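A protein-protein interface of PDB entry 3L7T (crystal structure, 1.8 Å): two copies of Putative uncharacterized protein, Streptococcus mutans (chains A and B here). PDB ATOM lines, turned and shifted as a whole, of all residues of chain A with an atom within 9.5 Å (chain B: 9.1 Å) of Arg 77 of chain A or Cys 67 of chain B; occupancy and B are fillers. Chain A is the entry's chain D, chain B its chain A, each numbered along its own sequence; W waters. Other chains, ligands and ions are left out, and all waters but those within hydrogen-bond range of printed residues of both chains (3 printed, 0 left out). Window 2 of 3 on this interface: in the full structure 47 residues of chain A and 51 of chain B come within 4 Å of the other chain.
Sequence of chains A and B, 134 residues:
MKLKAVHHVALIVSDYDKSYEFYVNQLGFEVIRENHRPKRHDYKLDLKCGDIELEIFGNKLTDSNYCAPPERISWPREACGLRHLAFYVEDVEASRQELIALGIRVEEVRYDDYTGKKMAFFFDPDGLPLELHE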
ATOM      1  N   ARG A  72      23.554  43.758 -10.348  1.00  0.00           N
ATOM      2  CA  ARG A  72      22.449  42.804 -10.434  1.00  0.00           C
ATOM      3  C   ARG A  72      22.979  41.427 -10.857  1.00  0.00           C
ATOM      4  O   ARG A  72      23.853  41.324 -11.723  1.00  0.00           O
ATOM      5  CB  ARG A  72      21.416  43.313 -11.445  1.00  0.00           C
ATOM      6  CG  ARG A  72      20.240  42.369 -11.667  1.00  0.00           C
ATOM      7  CD  ARG A  72      19.171  43.040 -12.545  1.00  0.00           C
ATOM      8  NE  ARG A  72      18.017  42.164 -12.753  1.00  0.00           N
ATOM      9  CZ  ARG A  72      17.986  41.129 -13.588  1.00  0.00           C
ATOM     10  NH1 ARG A  72      18.995  40.900 -14.432  1.00  0.00           N
ATOM     11  NH2 ARG A  72      16.869  40.425 -13.703  1.00  0.00           N
ATOM     12  N   ILE A  73      22.418  40.373 -10.271  1.00  0.00           N
ATOM     13  CA  ILE A  73      22.773  39.002 -10.659  1.00  0.00           C
ATOM     14  C   ILE A  73      21.968  38.586 -11.874  1.00  0.00           C
ATOM     15  O   ILE A  73      20.735  38.620 -11.855  1.00  0.00           O
ATOM     16  CB  ILE A  73      22.548  38.007  -9.498  1.00  0.00           C
ATOM     17  CG1 ILE A  73      23.339  38.430  -8.258  1.00  0.00           C
ATOM     18  CG2 ILE A  73      22.932  36.574  -9.916  1.00  0.00           C
ATOM     19  CD1 ILE A  73      24.809  38.644  -8.541  1.00  0.00           C
ATOM     20  N   SER A  74      22.676  38.241 -12.948  1.00  0.00           N
ATOM     21  CA  SER A  74      22.041  37.842 -14.191  1.00  0.00           C
ATOM     22  C   SER A  74      22.444  36.454 -14.682  1.00  0.00           C
ATOM     23  O   SER A  74      21.701  35.814 -15.412  1.00  0.00           O
ATOM     24  CB  SER A  74      22.303  38.901 -15.262  1.00  0.00           C
ATOM     25  OG  SER A  74      22.075  40.193 -14.704  1.00  0.00           O
ATOM     26  N   TRP A  75      23.632  35.985 -14.306  1.00  0.00           N
ATOM     27  CA  TRP A  75      24.129  34.730 -14.846  1.00  0.00           C
ATOM     28  C   TRP A  75      24.927  33.990 -13.776  1.00  0.00           C
ATOM     29  O   TRP A  75      25.666  34.621 -13.027  1.00  0.00           O
ATOM     30  CB  TRP A  75      25.006  34.996 -16.083  1.00  0.00           C
ATOM     31  CG  TRP A  75      25.228  33.764 -16.950  1.00  0.00           C
ATOM     32  CD1 TRP A  75      26.391  33.048 -17.077  1.00  0.00           C
ATOM     33  CD2 TRP A  75      24.266  33.115 -17.807  1.00  0.00           C
ATOM     34  NE1 TRP A  75      26.200  31.976 -17.924  1.00  0.00           N
ATOM     35  CE2 TRP A  75      24.914  32.004 -18.399  1.00  0.00           C
ATOM     36  CE3 TRP A  75      22.918  33.347 -18.106  1.00  0.00           C
ATOM     37  CZ2 TRP A  75      24.255  31.130 -19.278  1.00  0.00           C
ATOM     38  CZ3 TRP A  75      22.276  32.494 -19.006  1.00  0.00           C
ATOM     39  CH2 TRP A  75      22.938  31.390 -19.562  1.00  0.00           C
ATOM     40  N   PRO A  76      24.789  32.656 -13.706  1.00  0.00           N
ATOM     41  CA  PRO A  76      23.947  31.787 -14.566  1.00  0.00           C
ATOM     42  C   PRO A  76      22.417  31.853 -14.314  1.00  0.00           C
ATOM     43  O   PRO A  76      21.634  31.427 -15.181  1.00  0.00           O
ATOM     44  CB  PRO A  76      24.475  30.380 -14.246  1.00  0.00           C
ATOM     45  CG  PRO A  76      24.953  30.493 -12.790  1.00  0.00           C
ATOM     46  CD  PRO A  76      25.606  31.868 -12.758  1.00  0.00           C
ATOM     47  N   ARG A  77      22.010  32.246 -13.105  1.00  0.00           N
ATOM     48  CA  ARG A  77      20.589  32.368 -12.722  1.00  0.00           C
ATOM     49  C   ARG A  77      20.328  33.705 -11.998  1.00  0.00           C
ATOM     50  O   ARG A  77      21.132  34.144 -11.187  1.00  0.00           O
ATOM     51  CB  ARG A  77      20.198  31.189 -11.825  1.00  0.00           C
ATOM     52  CG  ARG A  77      20.190  29.887 -12.599  1.00  0.00           C
ATOM     53  CD  ARG A  77      20.031  28.653 -11.755  1.00  0.00           C
ATOM     54  NE  ARG A  77      19.999  27.473 -12.621  1.00  0.00           N
ATOM     55  CZ  ARG A  77      18.903  27.001 -13.213  1.00  0.00           C
ATOM     56  NH1 ARG A  77      17.720  27.586 -13.018  1.00  0.00           N
ATOM     57  NH2 ARG A  77      18.980  25.929 -13.984  1.00  0.00           N
ATOM     58  N   GLU A  78      19.223  34.377 -12.316  1.00  0.00           N
ATOM     59  CA  GLU A  78      18.846  35.558 -11.553  1.00  0.00           C
ATOM     60  C   GLU A  78      18.439  35.158 -10.147  1.00  0.00           C
ATOM     61  O   GLU A  78      17.989  34.022  -9.897  1.00  0.00           O
ATOM     62  CB  GLU A  78      17.695  36.300 -12.240  1.00  0.00           C
ATOM     63  CG  GLU A  78      18.058  36.815 -13.644  1.00  0.00           C
ATOM     64  CD  GLU A  78      16.823  37.036 -14.487  1.00  0.00           C
ATOM     65  OE1 GLU A  78      16.143  36.049 -14.835  1.00  0.00           O
ATOM     66  OE2 GLU A  78      16.541  38.187 -14.825  1.00  0.00           O
ATOM     67  N   ALA A  79      18.611  36.088  -9.221  1.00  0.00           N
ATOM     68  CA  ALA A  79      18.247  35.874  -7.822  1.00  0.00           C
ATOM     69  C   ALA A  79      16.739  35.872  -7.614  1.00  0.00           C
ATOM     70  O   ALA A  79      15.983  36.498  -8.402  1.00  0.00           O
ATOM     71  CB  ALA A  79      18.902  36.966  -6.939  1.00  0.00           C
ATOM     72  N   CYS A  80      16.328  35.360  -6.452  1.00  0.00           N
ATOM     73  CA  CYS A  80      14.992  35.596  -5.938  1.00  0.00           C
ATOM     74  C   CYS A  80      14.719  37.102  -5.878  1.00  0.00           C
ATOM     75  O   CYS A  80      15.607  37.898  -5.552  1.00  0.00           O
ATOM     76  CB  CYS A  80      14.850  35.038  -4.526  1.00  0.00           C
ATOM     77  SG  CYS A  80      14.759  33.208  -4.517  1.00  0.00           S
ATOM     78  N   ARG A  83      12.202  40.767 -10.741  1.00  0.00           N
ATOM     79  CA  ARG A  83      13.007  40.281 -11.818  1.00  0.00           C
ATOM     80  C   ARG A  83      13.039  41.319 -12.954  1.00  0.00           C
ATOM     81  O   ARG A  83      14.112  41.778 -13.343  1.00  0.00           O
ATOM     82  CB  ARG A  83      12.469  38.928 -12.284  1.00  0.00           C
ATOM     83  CG  ARG A  83      13.255  38.345 -13.426  1.00  0.00           C
ATOM     84  CD  ARG A  83      12.487  37.213 -14.102  1.00  0.00           C
ATOM     85  NE  ARG A  83      13.404  36.510 -14.996  1.00  0.00           N
ATOM     86  CZ  ARG A  83      13.049  35.516 -15.797  1.00  0.00           C
ATOM     87  NH1 ARG A  83      11.772  35.134 -15.870  1.00  0.00           N
ATOM     88  NH2 ARG A  83      13.958  34.952 -16.588  1.00  0.00           N
ATOM     89  N   ILE B  12      11.009  36.311  -9.113  1.00  0.00           N
ATOM     90  CA  ILE B  12      11.510  34.937  -8.992  1.00  0.00           C
ATOM     91  C   ILE B  12      11.358  34.466  -7.549  1.00  0.00           C
ATOM     92  O   ILE B  12      11.658  35.189  -6.618  1.00  0.00           O
ATOM     93  CB  ILE B  12      12.986  34.861  -9.429  1.00  0.00           C
ATOM     94  CG1 ILE B  12      13.051  35.070 -10.954  1.00  0.00           C
ATOM     95  CG2 ILE B  12      13.626  33.479  -9.017  1.00  0.00           C
ATOM     96  CD1 ILE B  12      14.429  35.082 -11.574  1.00  0.00           C
ATOM     97  N   VAL B  13      10.961  33.205  -7.366  1.00  0.00           N
ATOM     98  CA  VAL B  13      10.775  32.635  -6.034  1.00  0.00           C
ATOM     99  C   VAL B  13      11.573  31.320  -5.985  1.00  0.00           C
ATOM    100  O   VAL B  13      11.946  30.795  -7.033  1.00  0.00           O
ATOM    101  CB  VAL B  13       9.284  32.363  -5.696  1.00  0.00           C
ATOM    102  CG1 VAL B  13       8.450  33.683  -5.745  1.00  0.00           C
ATOM    103  CG2 VAL B  13       8.684  31.296  -6.625  1.00  0.00           C
ATOM    104  N   SER B  14      11.987  30.928  -4.788  1.00  0.00           N
ATOM    105  CA  SER B  14      12.819  29.733  -4.639  1.00  0.00           C
ATOM    106  C   SER B  14      11.947  28.467  -4.618  1.00  0.00           C
ATOM    107  O   SER B  14      12.357  27.422  -5.126  1.00  0.00           O
ATOM    108  CB  SER B  14      13.721  29.829  -3.382  1.00  0.00           C
ATOM    109  OG  SER B  14      12.941  29.765  -2.181  1.00  0.00           O
ATOM    110  N   ASP B  15      10.822  28.532  -3.913  1.00  0.00           N
ATOM    111  CA  ASP B  15       9.987  27.356  -3.718  1.00  0.00           C
ATOM    112  C   ASP B  15       8.612  27.657  -4.289  1.00  0.00           C
ATOM    113  O   ASP B  15       7.829  28.365  -3.667  1.00  0.00           O
ATOM    114  CB  ASP B  15       9.876  27.030  -2.214  1.00  0.00           C
ATOM    115  CG  ASP B  15       9.050  25.782  -1.938  1.00  0.00           C
ATOM    116  OD1 ASP B  15       7.941  25.629  -2.511  1.00  0.00           O
ATOM    117  OD2 ASP B  15       9.469  24.984  -1.069  1.00  0.00           O
ATOM    118  N   LYS B  39      12.394  23.805 -17.931  1.00  0.00           N
ATOM    119  CA  LYS B  39      13.566  24.523 -18.351  1.00  0.00           C
ATOM    120  C   LYS B  39      13.321  25.875 -19.039  1.00  0.00           C
ATOM    121  O   LYS B  39      13.774  26.914 -18.547  1.00  0.00           O
ATOM    122  CB  LYS B  39      14.470  23.621 -19.147  1.00  0.00           C
ATOM    123  CG  LYS B  39      14.002  23.242 -20.462  1.00  0.00           C
ATOM    124  CD  LYS B  39      15.084  22.393 -21.124  1.00  0.00           C
ATOM    125  CE  LYS B  39      14.604  21.592 -22.325  1.00  0.00           C
ATOM    126  NZ  LYS B  39      15.081  22.126 -23.621  1.00  0.00           N
ATOM    127  N   ARG B  40      12.605  25.896 -20.141  1.00  0.00           N
ATOM    128  CA  ARG B  40      12.366  27.169 -20.742  1.00  0.00           C
ATOM    129  C   ARG B  40      12.066  28.198 -19.665  1.00  0.00           C
ATOM    130  O   ARG B  40      12.784  29.149 -19.507  1.00  0.00           O
ATOM    131  CB  ARG B  40      11.267  27.142 -21.772  1.00  0.00           C
ATOM    132  CG  ARG B  40      11.007  28.499 -22.327  1.00  0.00           C
ATOM    133  CD  ARG B  40      10.805  28.455 -23.779  1.00  0.00           C
ATOM    134  NE  ARG B  40       9.726  27.560 -24.133  1.00  0.00           N
ATOM    135  CZ  ARG B  40       8.444  27.866 -24.068  1.00  0.00           C
ATOM    136  NH1 ARG B  40       8.060  29.033 -23.633  1.00  0.00           N
ATOM    137  NH2 ARG B  40       7.560  26.997 -24.436  1.00  0.00           N
ATOM    138  N   HIS B  41      10.994  28.005 -18.929  1.00  0.00           N
ATOM    139  CA  HIS B  41      10.691  28.947 -17.847  1.00  0.00           C
ATOM    140  C   HIS B  41      10.105  28.299 -16.603  1.00  0.00           C
ATOM    141  O   HIS B  41       9.558  28.995 -15.754  1.00  0.00           O
ATOM    142  CB  HIS B  41       9.806  30.103 -18.336  1.00  0.00           C
ATOM    143  CG  HIS B  41       8.400  29.702 -18.671  1.00  0.00           C
ATOM    144  ND1 HIS B  41       7.588  29.014 -17.793  1.00  0.00           N
ATOM    145  CD2 HIS B  41       7.630  29.989 -19.746  1.00  0.00           C
ATOM    146  CE1 HIS B  41       6.396  28.857 -18.332  1.00  0.00           C
ATOM    147  NE2 HIS B  41       6.398  29.426 -19.525  1.00  0.00           N
ATOM    148  N   ASP B  42      10.229  26.972 -16.488  1.00  0.00           N
ATOM    149  CA  ASP B  42       9.625  26.254 -15.360  1.00  0.00           C
ATOM    150  C   ASP B  42       8.193  26.728 -15.149  1.00  0.00           C
ATOM    151  O   ASP B  42       7.433  26.779 -16.139  1.00  0.00           O
ATOM    152  CB  ASP B  42      10.515  26.376 -14.127  1.00  0.00           C
ATOM    153  CG  ASP B  42      11.897  25.768 -14.364  1.00  0.00           C
ATOM    154  OD1 ASP B  42      11.947  24.690 -15.002  1.00  0.00           O
ATOM    155  OD2 ASP B  42      12.924  26.398 -13.989  1.00  0.00           O
ATOM    156  N   GLY B  58       9.107  30.298 -10.898  1.00  0.00           N
ATOM    157  CA  GLY B  58       9.879  29.508  -9.942  1.00  0.00           C
ATOM    158  C   GLY B  58       9.736  28.071 -10.344  1.00  0.00           C
ATOM    159  O   GLY B  58       9.117  27.755 -11.357  1.00  0.00           O
ATOM    160  N   ASN B  59      10.306  27.215  -9.529  1.00  0.00           N
ATOM    161  CA  ASN B  59      10.237  25.793  -9.796  1.00  0.00           C
ATOM    162  C   ASN B  59       9.926  25.070  -8.493  1.00  0.00           C
ATOM    163  O   ASN B  59      10.126  25.607  -7.409  1.00  0.00           O
ATOM    164  CB  ASN B  59      11.547  25.305 -10.408  1.00  0.00           C
ATOM    165  CG  ASN B  59      11.420  23.921 -11.032  1.00  0.00           C
ATOM    166  OD1 ASN B  59      10.323  23.405 -11.154  1.00  0.00           O
ATOM    167  ND2 ASN B  59      12.546  23.327 -11.443  1.00  0.00           N
ATOM    168  N   LYS B  60       9.336  23.878  -8.603  1.00  0.00           N
ATOM    169  CA  LYS B  60       8.866  23.148  -7.432  1.00  0.00           C
ATOM    170  C   LYS B  60      10.041  22.303  -6.956  1.00  0.00           C
ATOM    171  O   LYS B  60      10.827  21.878  -7.785  1.00  0.00           O
ATOM    172  CB  LYS B  60       7.725  22.217  -7.856  1.00  0.00           C
ATOM    173  CG  LYS B  60       6.423  22.914  -8.055  1.00  0.00           C
ATOM    174  CD  LYS B  60       5.369  22.006  -8.629  1.00  0.00           C
ATOM    175  CE  LYS B  60       4.104  22.802  -8.866  1.00  0.00           C
ATOM    176  NZ  LYS B  60       2.964  21.967  -9.351  1.00  0.00           N
ATOM    177  N   LEU B  61      10.163  22.089  -5.644  1.00  0.00           N
ATOM    178  CA  LEU B  61      11.343  21.403  -5.075  1.00  0.00           C
ATOM    179  C   LEU B  61      11.366  19.937  -5.502  1.00  0.00           C
ATOM    180  O   LEU B  61      12.420  19.310  -5.543  1.00  0.00           O
ATOM    181  CB  LEU B  61      11.327  21.474  -3.545  1.00  0.00           C
ATOM    182  CG  LEU B  61      12.038  22.609  -2.798  1.00  0.00           C
ATOM    183  CD1 LEU B  61      11.697  23.983  -3.351  1.00  0.00           C
ATOM    184  CD2 LEU B  61      11.649  22.525  -1.312  1.00  0.00           C
ATOM    185  N   THR B  62      10.193  19.420  -5.840  1.00  0.00           N
ATOM    186  CA  THR B  62      10.033  18.049  -6.295  1.00  0.00           C
ATOM    187  C   THR B  62      10.380  17.873  -7.774  1.00  0.00           C
ATOM    188  O   THR B  62      10.527  16.746  -8.230  1.00  0.00           O
ATOM    189  CB  THR B  62       8.586  17.558  -6.073  1.00  0.00           C
ATOM    190  OG1 THR B  62       7.668  18.452  -6.715  1.00  0.00           O
ATOM    191  CG2 THR B  62       8.248  17.498  -4.593  1.00  0.00           C
ATOM    192  N   ASP B  63      10.457  18.970  -8.533  1.00  0.00           N
ATOM    193  CA  ASP B  63      10.789  18.887  -9.959  1.00  0.00           C
ATOM    194  C   ASP B  63      12.138  18.205 -10.131  1.00  0.00           C
ATOM    195  O   ASP B  63      13.076  18.458  -9.369  1.00  0.00           O
ATOM    196  CB  ASP B  63      10.842  20.275 -10.599  1.00  0.00           C
ATOM    197  CG  ASP B  63      10.959  20.219 -12.126  1.00  0.00           C
ATOM    198  OD1 ASP B  63       9.934  19.962 -12.791  1.00  0.00           O
ATOM    199  OD2 ASP B  63      12.059  20.493 -12.664  1.00  0.00           O
ATOM    200  N   SER B  64      12.252  17.368 -11.153  1.00  0.00           N
ATOM    201  CA  SER B  64      13.451  16.552 -11.306  1.00  0.00           C
ATOM    202  C   SER B  64      14.688  17.378 -11.669  1.00  0.00           C
ATOM    203  O   SER B  64      15.819  16.935 -11.442  1.00  0.00           O
ATOM    204  CB  SER B  64      13.226  15.431 -12.322  1.00  0.00           C
ATOM    205  OG  SER B  64      13.126  15.958 -13.631  1.00  0.00           O
ATOM    206  N   ASN B  65      14.473  18.591 -12.180  1.00  0.00           N
ATOM    207  CA  ASN B  65      15.583  19.484 -12.526  1.00  0.00           C
ATOM    208  C   ASN B  65      15.640  20.767 -11.672  1.00  0.00           C
ATOM    209  O   ASN B  65      16.091  21.815 -12.136  1.00  0.00           O
ATOM    210  CB  ASN B  65      15.544  19.839 -14.015  1.00  0.00           C
ATOM    211  CG  ASN B  65      15.763  18.621 -14.913  1.00  0.00           C
ATOM    212  OD1 ASN B  65      14.956  18.339 -15.802  1.00  0.00           O
ATOM    213  ND2 ASN B  65      16.829  17.866 -14.644  1.00  0.00           N
ATOM    214  N   TYR B  66      15.225  20.654 -10.420  1.00  0.00           N
ATOM    215  CA  TYR B  66      15.260  21.776  -9.486  1.00  0.00           C
ATOM    216  C   TYR B  66      16.668  22.317  -9.215  1.00  0.00           C
ATOM    217  O   TYR B  66      17.587  21.564  -8.875  1.00  0.00           O
ATOM    218  CB  TYR B  66      14.606  21.389  -8.178  1.00  0.00           C
ATOM    219  CG  TYR B  66      14.549  22.548  -7.227  1.00  0.00           C
ATOM    220  CD1 TYR B  66      13.575  23.534  -7.364  1.00  0.00           C
ATOM    221  CD2 TYR B  66      15.540  22.729  -6.278  1.00  0.00           C
ATOM    222  CE1 TYR B  66      13.526  24.601  -6.494  1.00  0.00           C
ATOM    223  CE2 TYR B  66      15.523  23.810  -5.437  1.00  0.00           C
ATOM    224  CZ  TYR B  66      14.526  24.754  -5.556  1.00  0.00           C
ATOM    225  OH  TYR B  66      14.524  25.834  -4.695  1.00  0.00           O
ATOM    226  N   CYS B  67      16.840  23.624  -9.393  1.00  0.00           N
ATOM    227  CA  CYS B  67      18.084  24.303  -9.005  1.00  0.00           C
ATOM    228  C   CYS B  67      17.659  25.583  -8.294  1.00  0.00           C
ATOM    229  O   CYS B  67      16.993  26.414  -8.896  1.00  0.00           O
ATOM    230  CB  CYS B  67      18.878  24.732 -10.237  1.00  0.00           C
ATOM    231  SG  CYS B  67      19.642  23.423 -11.172  1.00  0.00           S
ATOM    232  N   ALA B  68      17.933  25.684  -7.001  1.00  0.00           N
ATOM    233  CA  ALA B  68      17.498  26.850  -6.245  1.00  0.00           C
ATOM    234  C   ALA B  68      18.147  28.120  -6.800  1.00  0.00           C
ATOM    235  O   ALA B  68      19.359  28.157  -7.009  1.00  0.00           O
ATOM    236  CB  ALA B  68      17.846  26.662  -4.768  1.00  0.00           C
ATOM    237  N   PRO B  69      17.359  29.196  -7.009  1.00  0.00           N
ATOM    238  CA  PRO B  69      18.026  30.438  -7.424  1.00  0.00           C
ATOM    239  C   PRO B  69      18.785  31.077  -6.259  1.00  0.00           C
ATOM    240  O   PRO B  69      18.469  30.783  -5.094  1.00  0.00           O
ATOM    241  CB  PRO B  69      16.860  31.340  -7.852  1.00  0.00           C
ATOM    242  CG  PRO B  69      15.677  30.822  -7.087  1.00  0.00           C
ATOM    243  CD  PRO B  69      15.895  29.342  -6.888  1.00  0.00           C
ATOM    244  N   PRO B  70      19.746  31.980  -6.552  1.00  0.00           N
ATOM    245  CA  PRO B  70      20.429  32.642  -5.436  1.00  0.00           C
ATOM    246  C   PRO B  70      19.468  33.430  -4.560  1.00  0.00           C
ATOM    247  O   PRO B  70      18.351  33.777  -5.000  1.00  0.00           O
ATOM    248  CB  PRO B  70      21.420  33.588  -6.112  1.00  0.00           C
ATOM    249  CG  PRO B  70      21.457  33.204  -7.553  1.00  0.00           C
ATOM    250  CD  PRO B  70      20.216  32.444  -7.865  1.00  0.00           C
ATOM    251  N   GLU B  71      19.868  33.653  -3.314  1.00  0.00           N
ATOM    252  CA  GLU B  71      19.089  34.479  -2.401  1.00  0.00           C
ATOM    253  C   GLU B  71      19.176  35.944  -2.826  1.00  0.00           C
ATOM    254  O   GLU B  71      20.149  36.379  -3.452  1.00  0.00           O
ATOM    255  CB  GLU B  71      19.570  34.315  -0.953  1.00  0.00           C
ATOM    256  CG  GLU B  71      19.151  32.983  -0.361  1.00  0.00           C
ATOM    257  CD  GLU B  71      19.622  32.758   1.078  1.00  0.00           C
ATOM    258  OE1 GLU B  71      20.503  33.499   1.586  1.00  0.00           O
ATOM    259  OE2 GLU B  71      19.097  31.810   1.696  1.00  0.00           O
HETATM  260  O   HOH W   1      16.972  30.796  -2.884  1.00  0.00           O
HETATM  261  O   HOH W   2      16.845  29.179 -10.631  1.00  0.00           O
HETATM  262  O   HOH W   3      15.509  25.694 -13.382  1.00  0.00           O
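No position is printed for both chains.
Of the 14 pairs that touch across the chains among the printed residues, none has its exchanged pair printed and touching as well.
SG of Cys 80 of chain A is in hydrogen-bond range of N of Ser 14 of chain B.
The backbone carbonyl oxygen of Pro 70 of chain B lies within hydrogen-bond range of the backbone NH of Cys 80 of chain A, 3.0 Å away.
Arg 77 of chain A touches Cys 67 of chain B (CZ to CB, 3.7 Å).
Pro 70 of chain B touches Arg 77 of chain A (CG to O, 3.8 Å).
Glu 78 of chain A touches Ile 12 of chain B (CB to CD1, 3.5 Å).
Pro 69 of chain B touches Glu 78 of chain A (CB to O, 3.6 Å).
Ala 79 of chain A touches Ile 12 of chain B.
Pro 70 of chain B touches Ala 79 of chain A.
CB of Ala 79 of chain A touches O of Glu 71 of chain B (3.7 Å).
O of Ile 12 of chain B touches CA of Cys 80 of chain A (3.4 Å).
Cys 80 of chain A touches Val 13 of chain B.
Pro 69 of chain B touches Cys 80 of chain A.
Of the 10 printed residues of chain A, 5 touch a printed residue of chain B.
Hydrophobic or aromatic side chains of chain A within 4 Å of the printed part of chain B: Ala 79.
Of the 22 printed residues of chain B, 7 touch a printed residue of chain A.
Hydrophobic or aromatic side chains of chain B within 4 Å of the printed part of chain A: Ile 12, Pro 69 and Pro 70.
Along chain B the printed residues that touch a printed residue of chain A span positions 12 to 71.
Among the printed residues, 14 pairs touch across the chains.
Among the printed residues, no Asp or Glu carboxylate lies within 4 Å of a Lys or Arg side-chain nitrogen of the other chain.
OE1 of Glu 78 of chain A lies within salt-bridge range of NE of Arg 83 of chain A (2.8 Å).
The guanidinium group of Arg 72 of chain A sits at hydrogen-bond distance from the backbone carbonyl oxygen of Arg 83 of chain A (3.1 Å).
The backbone carbonyl oxygen (O) of Ser 14 of chain B sits at hydrogen-bond distance from the side-chain hydroxyl (OH) of Tyr 66 of chain B, at 2.7 Å.
The guanidinium group of Arg 72 of chain A is in salt-bridge range of the side-chain carboxylate of Glu 78 of chain A (2.5 Å).
Printed residues of chain B within 4 Å of Arg 77 of chain A: Cys 67 and Pro 70.
Cys 67 of chain B touches just one residue of chain A: Arg 77.
No residue of chain B comes within 4 Å of Pro 76 of chain A.
No residue of chain A comes within 4 Å of Tyr 66 of chain B.
No residue of chain A comes within 4 Å of Ala 68 of chain B.
Of the printed residues of chain B, Arg 83 of chain A touches Ile 12.
Of the printed residues of chain A, Ile 12 of chain B touches Glu 78, Ala 79, Cys 80 and Arg 83.
Arg 40 of chain B touches none of the printed residues of chain A.
The nearest residue of chain B that does not touch Arg 77 of chain A is Ala 68 of chain B (4.8 Å).
Water W1 lies within hydrogen-bond range of O of Pro 69 of chain B (2.7 Å) and SG of Cys 80 of chain A (3.7 Å).
Water W3 lies within hydrogen-bond range of the side-chain carboxylate (OD2) of Asp 42 of chain B and the guanidinium group (NH1) of Arg 77 of chain A.
Water W2 lies within hydrogen-bond range of NH1 of Arg 77 of chain A and O of Cys 67 of chain B.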
